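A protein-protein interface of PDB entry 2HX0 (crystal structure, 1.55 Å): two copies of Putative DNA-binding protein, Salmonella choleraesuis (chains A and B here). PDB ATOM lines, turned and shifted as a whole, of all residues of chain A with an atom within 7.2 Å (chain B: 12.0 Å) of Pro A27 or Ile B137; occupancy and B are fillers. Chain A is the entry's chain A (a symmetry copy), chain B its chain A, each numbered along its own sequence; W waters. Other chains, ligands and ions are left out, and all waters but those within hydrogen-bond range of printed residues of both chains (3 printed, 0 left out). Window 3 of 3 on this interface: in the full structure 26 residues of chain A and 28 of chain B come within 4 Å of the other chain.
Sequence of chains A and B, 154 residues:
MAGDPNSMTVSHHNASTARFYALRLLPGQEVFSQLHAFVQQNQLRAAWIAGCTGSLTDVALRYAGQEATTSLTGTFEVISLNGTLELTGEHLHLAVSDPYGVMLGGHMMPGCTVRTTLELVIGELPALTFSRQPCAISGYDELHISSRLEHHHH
No residue of chain B comes within 4 Å of Leu A26. Pro A27 touches just one residue of chain B: Ile B137 (3.7 Å). No residue of chain B comes within 4 Å of Gly A28. No residue of chain B comes within 4 Å of Gln A29. No residue of chain B comes within 4 Å of Val A114. Printed residues of chain B within 4 Å of Thr A116: Ser B138 and Glu B142. Printed residues of chain A within 4 Å of Ile B137: Pro A27. Of the printed residues of chain A, Ser B138 touches Thr A116 (3.7 Å). Of the printed residues of chain A, Leu B143 touches Arg A24.
Water W1 lies within hydrogen-bond range of the side-chain carboxylate (OE1) of Glu B142 (2.6 Å), the side-chain hydroxyl (OG1) of Thr A117 (2.8 Å) and the backbone NH (N) of Leu B143 (2.8 Å). Water W2 lies within hydrogen-bond range of the side-chain carboxylate (OE2) of Glu B142 (2.7 Å) and the side-chain hydroxyl (OG1) of Thr A116 (2.7 Å). Water W3 lies within hydrogen-bond range of O of Leu B143 (2.9 Å) and NH1 of Arg A24 (3.0 Å).
The backbone carbonyl oxygen (O) of Gln B133 sits at hydrogen-bond distance from the backbone NH (N) of Glu B142. SG of Cys B135 lies close to N of Ile B137 (3.4 Å). The backbone NH of Cys B135 lies within hydrogen-bond range of the backbone carbonyl oxygen of Tyr B140, 2.9 Å away. The side-chain hydroxyl of Ser B138 sits at hydrogen-bond distance from the backbone NH of Tyr B140 (3.2 Å). OG of Ser B138 lies within hydrogen-bond range of OE2 of Glu B142, 2.7 Å away. The guanidinium group (NH2) of Arg A24 lies within hydrogen-bond range of the backbone carbonyl oxygen (O) of Thr A116 (3.0 Å).
SG of Cys B135 lies within hydrogen-bond range of NH1 of Arg A24 (3.4 Å).
Printed residues of chain A that touch a printed residue of chain B: Arg A24, Pro A27, Thr A116 and Thr A117. Among the printed residues, 8 pairs touch across the chains.
No position is printed for both chains. Of the 8 pairs that touch across the chains among the printed residues, none has its exchanged pair printed and touching as well.
Arg A24 touches Glu B142. CD of Arg A24 touches O of Leu B143, at 3.8 Å. Pro A27 touches Ile B137 (CG to CG2, 3.7 Å). Thr A116 touches Ser B138. Thr A116 touches Glu B142. Thr A117 touches His B91 (CG2 to CE1, 3.9 Å). CB of Thr A117 touches OE1 of Glu B142 (3.5 Å).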
ATOM      1  N   ARG A  24      30.801  16.826 -11.719  1.00  0.00           N
ATOM      2  CA  ARG A  24      30.356  16.863 -13.097  1.00  0.00           C
ATOM      3  C   ARG A  24      30.910  18.109 -13.762  1.00  0.00           C
ATOM      4  O   ARG A  24      30.726  19.215 -13.255  1.00  0.00           O
ATOM      5  CB  ARG A  24      28.833  16.904 -13.166  1.00  0.00           C
ATOM      6  CG  ARG A  24      28.316  16.927 -14.588  1.00  0.00           C
ATOM      7  CD  ARG A  24      27.297  18.023 -14.798  1.00  0.00           C
ATOM      8  NE  ARG A  24      27.090  18.268 -16.222  1.00  0.00           N
ATOM      9  CZ  ARG A  24      26.312  19.227 -16.713  1.00  0.00           C
ATOM     10  NH1 ARG A  24      25.656  20.040 -15.894  1.00  0.00           N
ATOM     11  NH2 ARG A  24      26.194  19.376 -18.025  1.00  0.00           N
ATOM     12  N   LEU A  25      31.590  17.930 -14.890  1.00  0.00           N
ATOM     13  CA  LEU A  25      32.144  19.068 -15.616  1.00  0.00           C
ATOM     14  C   LEU A  25      31.112  19.559 -16.622  1.00  0.00           C
ATOM     15  O   LEU A  25      30.266  18.791 -17.088  1.00  0.00           O
ATOM     16  CB  LEU A  25      33.440  18.677 -16.321  1.00  0.00           C
ATOM     17  CG  LEU A  25      34.545  18.135 -15.400  1.00  0.00           C
ATOM     18  CD1 LEU A  25      35.826  17.993 -16.206  1.00  0.00           C
ATOM     19  CD2 LEU A  25      34.772  19.073 -14.211  1.00  0.00           C
ATOM     20  N   LEU A  26      31.199  20.841 -16.956  1.00  0.00           N
ATOM     21  CA  LEU A  26      30.251  21.481 -17.861  1.00  0.00           C
ATOM     22  C   LEU A  26      30.704  21.622 -19.311  1.00  0.00           C
ATOM     23  O   LEU A  26      31.893  21.570 -19.613  1.00  0.00           O
ATOM     24  CB  LEU A  26      29.906  22.874 -17.326  1.00  0.00           C
ATOM     25  CG  LEU A  26      29.437  22.977 -15.874  1.00  0.00           C
ATOM     26  CD1 LEU A  26      29.145  24.436 -15.543  1.00  0.00           C
ATOM     27  CD2 LEU A  26      28.202  22.125 -15.666  1.00  0.00           C
ATOM     28  N   PRO A  27      29.743  21.813 -20.229  1.00  0.00           N
ATOM     29  CA  PRO A  27      30.059  21.969 -21.650  1.00  0.00           C
ATOM     30  C   PRO A  27      31.090  23.076 -21.870  1.00  0.00           C
ATOM     31  O   PRO A  27      31.017  24.138 -21.246  1.00  0.00           O
ATOM     32  CB  PRO A  27      28.707  22.314 -22.261  1.00  0.00           C
ATOM     33  CG  PRO A  27      27.755  21.520 -21.413  1.00  0.00           C
ATOM     34  CD  PRO A  27      28.283  21.783 -20.018  1.00  0.00           C
ATOM     35  N   GLY A  28      32.057  22.810 -22.742  1.00  0.00           N
ATOM     36  CA  GLY A  28      33.074  23.799 -23.049  1.00  0.00           C
ATOM     37  C   GLY A  28      34.301  23.815 -22.164  1.00  0.00           C
ATOM     38  O   GLY A  28      35.322  24.392 -22.535  1.00  0.00           O
ATOM     39  N   GLN A  29      34.222  23.184 -20.998  1.00  0.00           N
ATOM     40  CA  GLN A  29      35.368  23.175 -20.103  1.00  0.00           C
ATOM     41  C   GLN A  29      36.441  22.203 -20.581  1.00  0.00           C
ATOM     42  O   GLN A  29      36.146  21.162 -21.175  1.00  0.00           O
ATOM     43  CB  GLN A  29      34.934  22.822 -18.674  1.00  0.00           C
ATOM     44  CG  GLN A  29      33.950  23.815 -18.055  1.00  0.00           C
ATOM     45  CD  GLN A  29      33.708  23.556 -16.579  1.00  0.00           C
ATOM     46  OE1 GLN A  29      33.415  22.432 -16.176  1.00  0.00           O
ATOM     47  NE2 GLN A  29      33.823  24.600 -15.765  1.00  0.00           N
ATOM     48  N   GLU A  30      37.692  22.566 -20.331  1.00  0.00           N
ATOM     49  CA  GLU A  30      38.832  21.745 -20.716  1.00  0.00           C
ATOM     50  C   GLU A  30      39.118  20.816 -19.532  1.00  0.00           C
ATOM     51  O   GLU A  30      39.246  21.265 -18.393  1.00  0.00           O
ATOM     52  CB  GLU A  30      40.020  22.658 -21.036  1.00  0.00           C
ATOM     53  CG  GLU A  30      41.206  21.983 -21.706  1.00  0.00           C
ATOM     54  CD  GLU A  30      42.095  21.277 -20.715  1.00  0.00           C
ATOM     55  OE1 GLU A  30      42.327  21.848 -19.630  1.00  0.00           O
ATOM     56  OE2 GLU A  30      42.569  20.162 -21.018  1.00  0.00           O
ATOM     57  N   THR A 113      38.004  18.970 -24.586  1.00  0.00           N
ATOM     58  CA  THR A 113      36.911  19.813 -24.115  1.00  0.00           C
ATOM     59  C   THR A 113      35.591  19.060 -24.008  1.00  0.00           C
ATOM     60  O   THR A 113      35.235  18.275 -24.884  1.00  0.00           O
ATOM     61  CB  THR A 113      36.718  21.045 -25.026  1.00  0.00           C
ATOM     62  OG1 THR A 113      36.389  20.621 -26.353  1.00  0.00           O
ATOM     63  CG2 THR A 113      37.996  21.871 -25.070  1.00  0.00           C
ATOM     64  N   VAL A 114      34.872  19.308 -22.917  1.00  0.00           N
ATOM     65  CA  VAL A 114      33.589  18.662 -22.658  1.00  0.00           C
ATOM     66  C   VAL A 114      32.520  19.068 -23.669  1.00  0.00           C
ATOM     67  O   VAL A 114      32.388  20.245 -24.020  1.00  0.00           O
ATOM     68  CB  VAL A 114      33.096  19.009 -21.234  1.00  0.00           C
ATOM     69  CG1 VAL A 114      31.746  18.358 -20.957  1.00  0.00           C
ATOM     70  CG2 VAL A 114      34.121  18.542 -20.217  1.00  0.00           C
ATOM     71  N   ARG A 115      31.748  18.090 -24.135  1.00  0.00           N
ATOM     72  CA  ARG A 115      30.686  18.366 -25.093  1.00  0.00           C
ATOM     73  C   ARG A 115      29.391  18.652 -24.338  1.00  0.00           C
ATOM     74  O   ARG A 115      28.904  19.781 -24.344  1.00  0.00           O
ATOM     75  CB  ARG A 115      30.509  17.178 -26.047  1.00  0.00           C
ATOM     76  CG  ARG A 115      29.538  17.436 -27.193  1.00  0.00           C
ATOM     77  CD  ARG A 115      29.918  16.614 -28.417  1.00  0.00           C
ATOM     78  NE  ARG A 115      29.928  15.175 -28.153  1.00  0.00           N
ATOM     79  CZ  ARG A 115      28.835  14.431 -28.020  1.00  0.00           C
ATOM     80  NH1 ARG A 115      27.633  14.985 -28.127  1.00  0.00           N
ATOM     81  NH2 ARG A 115      28.941  13.129 -27.779  1.00  0.00           N
ATOM     82  N   THR A 116      28.844  17.636 -23.676  1.00  0.00           N
ATOM     83  CA  THR A 116      27.619  17.819 -22.910  1.00  0.00           C
ATOM     84  C   THR A 116      27.871  17.638 -21.418  1.00  0.00           C
ATOM     85  O   THR A 116      27.231  18.292 -20.595  1.00  0.00           O
ATOM     86  CB  THR A 116      26.503  16.832 -23.338  1.00  0.00           C
ATOM     87  OG1 THR A 116      26.918  15.487 -23.076  1.00  0.00           O
ATOM     88  CG2 THR A 116      26.190  16.993 -24.817  1.00  0.00           C
ATOM     89  N   THR A 117      28.813  16.768 -21.063  1.00  0.00           N
ATOM     90  CA  THR A 117      29.090  16.521 -19.654  1.00  0.00           C
ATOM     91  C   THR A 117      30.278  15.583 -19.463  1.00  0.00           C
ATOM     92  O   THR A 117      30.696  14.891 -20.385  1.00  0.00           O
ATOM     93  CB  THR A 117      27.863  15.849 -18.970  1.00  0.00           C
ATOM     94  OG1 THR A 117      28.020  15.870 -17.546  1.00  0.00           O
ATOM     95  CG2 THR A 117      27.749  14.389 -19.407  1.00  0.00           C
ATOM     96  N   LEU A 118      30.833  15.588 -18.258  1.00  0.00           N
ATOM     97  CA  LEU A 118      31.895  14.654 -17.907  1.00  0.00           C
ATOM     98  C   LEU A 118      31.649  14.354 -16.438  1.00  0.00           C
ATOM     99  O   LEU A 118      31.797  15.225 -15.583  1.00  0.00           O
ATOM    100  CB  LEU A 118      33.298  15.230 -18.105  1.00  0.00           C
ATOM    101  CG  LEU A 118      34.314  14.077 -18.023  1.00  0.00           C
ATOM    102  CD1 LEU A 118      34.168  13.191 -19.261  1.00  0.00           C
ATOM    103  CD2 LEU A 118      35.733  14.611 -17.923  1.00  0.00           C
ATOM    104  N   HIS B  91      24.018   6.528 -16.195  1.00  0.00           N
ATOM    105  CA  HIS B  91      24.746   7.006 -17.365  1.00  0.00           C
ATOM    106  C   HIS B  91      25.920   6.050 -17.480  1.00  0.00           C
ATOM    107  O   HIS B  91      26.924   6.205 -16.785  1.00  0.00           O
ATOM    108  CB  HIS B  91      25.236   8.446 -17.166  1.00  0.00           C
ATOM    109  CG  HIS B  91      25.796   9.067 -18.410  1.00  0.00           C
ATOM    110  ND1 HIS B  91      26.238  10.371 -18.461  1.00  0.00           N
ATOM    111  CD2 HIS B  91      25.984   8.558 -19.651  1.00  0.00           C
ATOM    112  CE1 HIS B  91      26.672  10.642 -19.680  1.00  0.00           C
ATOM    113  NE2 HIS B  91      26.528   9.558 -20.422  1.00  0.00           N
ATOM    114  N   GLN B 133      19.071  16.249 -13.138  1.00  0.00           N
ATOM    115  CA  GLN B 133      18.348  17.510 -13.209  1.00  0.00           C
ATOM    116  C   GLN B 133      18.664  18.212 -14.520  1.00  0.00           C
ATOM    117  O   GLN B 133      19.782  18.129 -15.026  1.00  0.00           O
ATOM    118  CB  GLN B 133      18.757  18.405 -12.040  1.00  0.00           C
ATOM    119  CG  GLN B 133      18.700  17.720 -10.685  1.00  0.00           C
ATOM    120  CD  GLN B 133      17.288  17.421 -10.229  1.00  0.00           C
ATOM    121  OE1 GLN B 133      17.085  16.737  -9.226  1.00  0.00           O
ATOM    122  NE2 GLN B 133      16.302  17.937 -10.956  1.00  0.00           N
ATOM    123  N   PRO B 134      17.682  18.926 -15.086  1.00  0.00           N
ATOM    124  CA  PRO B 134      17.915  19.626 -16.350  1.00  0.00           C
ATOM    125  C   PRO B 134      19.021  20.675 -16.294  1.00  0.00           C
ATOM    126  O   PRO B 134      19.046  21.536 -15.410  1.00  0.00           O
ATOM    127  CB  PRO B 134      16.544  20.227 -16.670  1.00  0.00           C
ATOM    128  CG  PRO B 134      15.934  20.424 -15.321  1.00  0.00           C
ATOM    129  CD  PRO B 134      16.311  19.157 -14.598  1.00  0.00           C
ATOM    130  N   CYS B 135      19.947  20.577 -17.242  1.00  0.00           N
ATOM    131  CA  CYS B 135      21.053  21.514 -17.349  1.00  0.00           C
ATOM    132  C   CYS B 135      20.696  22.495 -18.461  1.00  0.00           C
ATOM    133  O   CYS B 135      20.455  22.092 -19.597  1.00  0.00           O
ATOM    134  CB  CYS B 135      22.346  20.775 -17.710  1.00  0.00           C
ATOM    135  SG  CYS B 135      23.772  21.853 -18.019  1.00  0.00           S
ATOM    136  N   ALA B 136      20.650  23.780 -18.131  1.00  0.00           N
ATOM    137  CA  ALA B 136      20.311  24.803 -19.113  1.00  0.00           C
ATOM    138  C   ALA B 136      21.395  24.942 -20.177  1.00  0.00           C
ATOM    139  O   ALA B 136      21.147  25.466 -21.264  1.00  0.00           O
ATOM    140  CB  ALA B 136      20.094  26.138 -18.413  1.00  0.00           C
ATOM    141  N   ILE B 137      22.594  24.467 -19.861  1.00  0.00           N
ATOM    142  CA  ILE B 137      23.714  24.557 -20.784  1.00  0.00           C
ATOM    143  C   ILE B 137      23.715  23.451 -21.835  1.00  0.00           C
ATOM    144  O   ILE B 137      23.834  23.728 -23.027  1.00  0.00           O
ATOM    145  CB  ILE B 137      25.057  24.513 -20.023  1.00  0.00           C
ATOM    146  CG1 ILE B 137      25.029  25.507 -18.858  1.00  0.00           C
ATOM    147  CG2 ILE B 137      26.201  24.851 -20.966  1.00  0.00           C
ATOM    148  CD1 ILE B 137      24.284  25.050 -17.630  1.00  0.00           C
ATOM    149  N   SER B 138      23.571  22.201 -21.399  1.00  0.00           N
ATOM    150  CA  SER B 138      23.576  21.072 -22.326  1.00  0.00           C
ATOM    151  C   SER B 138      22.208  20.809 -22.941  1.00  0.00           C
ATOM    152  O   SER B 138      22.111  20.279 -24.047  1.00  0.00           O
ATOM    153  CB  SER B 138      24.048  19.803 -21.614  1.00  0.00           C
ATOM    154  OG  SER B 138      23.047  19.311 -20.738  1.00  0.00           O
ATOM    155  N   GLY B 139      21.153  21.173 -22.219  1.00  0.00           N
ATOM    156  CA  GLY B 139      19.809  20.959 -22.723  1.00  0.00           C
ATOM    157  C   GLY B 139      19.277  19.575 -22.403  1.00  0.00           C
ATOM    158  O   GLY B 139      18.230  19.168 -22.913  1.00  0.00           O
ATOM    159  N   TYR B 140      20.001  18.845 -21.562  1.00  0.00           N
ATOM    160  CA  TYR B 140      19.601  17.496 -21.167  1.00  0.00           C
ATOM    161  C   TYR B 140      19.658  17.389 -19.652  1.00  0.00           C
ATOM    162  O   TYR B 140      20.221  18.257 -18.988  1.00  0.00           O
ATOM    163  CB  TYR B 140      20.560  16.459 -21.759  1.00  0.00           C
ATOM    164  CG  TYR B 140      20.685  16.490 -23.263  1.00  0.00           C
ATOM    165  CD1 TYR B 140      19.622  16.112 -24.078  1.00  0.00           C
ATOM    166  CD2 TYR B 140      21.876  16.878 -23.871  1.00  0.00           C
ATOM    167  CE1 TYR B 140      19.743  16.116 -25.474  1.00  0.00           C
ATOM    168  CE2 TYR B 140      22.008  16.888 -25.264  1.00  0.00           C
ATOM    169  CZ  TYR B 140      20.939  16.505 -26.059  1.00  0.00           C
ATOM    170  OH  TYR B 140      21.065  16.511 -27.434  1.00  0.00           O
ATOM    171  N   ASP B 141      19.072  16.329 -19.099  1.00  0.00           N
ATOM    172  CA  ASP B 141      19.118  16.129 -17.657  1.00  0.00           C
ATOM    173  C   ASP B 141      20.517  15.595 -17.374  1.00  0.00           C
ATOM    174  O   ASP B 141      20.934  14.595 -17.955  1.00  0.00           O
ATOM    175  CB  ASP B 141      18.061  15.115 -17.213  1.00  0.00           C
ATOM    176  CG  ASP B 141      16.646  15.586 -17.493  1.00  0.00           C
ATOM    177  OD1 ASP B 141      16.349  16.772 -17.239  1.00  0.00           O
ATOM    178  OD2 ASP B 141      15.831  14.763 -17.959  1.00  0.00           O
ATOM    179  N   GLU B 142      21.240  16.272 -16.490  1.00  0.00           N
ATOM    180  CA  GLU B 142      22.609  15.887 -16.166  1.00  0.00           C
ATOM    181  C   GLU B 142      22.775  15.530 -14.697  1.00  0.00           C
ATOM    182  O   GLU B 142      21.906  15.810 -13.875  1.00  0.00           O
ATOM    183  CB  GLU B 142      23.559  17.031 -16.521  1.00  0.00           C
ATOM    184  CG  GLU B 142      23.451  17.504 -17.966  1.00  0.00           C
ATOM    185  CD  GLU B 142      23.948  16.479 -18.968  1.00  0.00           C
ATOM    186  OE1 GLU B 142      24.445  15.414 -18.543  1.00  0.00           O
ATOM    187  OE2 GLU B 142      23.847  16.739 -20.189  1.00  0.00           O
ATOM    188  N   LEU B 143      23.907  14.915 -14.377  1.00  0.00           N
ATOM    189  CA  LEU B 143      24.187  14.502 -13.014  1.00  0.00           C
ATOM    190  C   LEU B 143      24.213  15.649 -12.012  1.00  0.00           C
ATOM    191  O   LEU B 143      24.912  16.646 -12.199  1.00  0.00           O
ATOM    192  CB  LEU B 143      25.521  13.751 -12.961  1.00  0.00           C
ATOM    193  CG  LEU B 143      25.949  13.263 -11.575  1.00  0.00           C
ATOM    194  CD1 LEU B 143      24.960  12.212 -11.065  1.00  0.00           C
ATOM    195  CD2 LEU B 143      27.351  12.679 -11.661  1.00  0.00           C
ATOM    196  N   HIS B 144      23.440  15.490 -10.943  1.00  0.00           N
ATOM    197  CA  HIS B 144      23.374  16.474  -9.873  1.00  0.00           C
ATOM    198  C   HIS B 144      23.784  15.725  -8.613  1.00  0.00           C
ATOM    199  O   HIS B 144      23.281  14.636  -8.343  1.00  0.00           O
ATOM    200  CB  HIS B 144      21.948  17.019  -9.730  1.00  0.00           C
ATOM    201  CG  HIS B 144      21.773  17.948  -8.569  1.00  0.00           C
ATOM    202  ND1 HIS B 144      22.520  19.096  -8.416  1.00  0.00           N
ATOM    203  CD2 HIS B 144      20.942  17.895  -7.501  1.00  0.00           C
ATOM    204  CE1 HIS B 144      22.158  19.709  -7.303  1.00  0.00           C
ATOM    205  NE2 HIS B 144      21.203  19.002  -6.729  1.00  0.00           N
HETATM  206  O   HOH W   1      25.761  14.522 -16.505  1.00  0.00           O
HETATM  207  O   HOH W   2      24.851  14.570 -21.520  1.00  0.00           O
HETATM  208  O   HOH W   3      24.196  19.156 -13.472  1.00  0.00           O
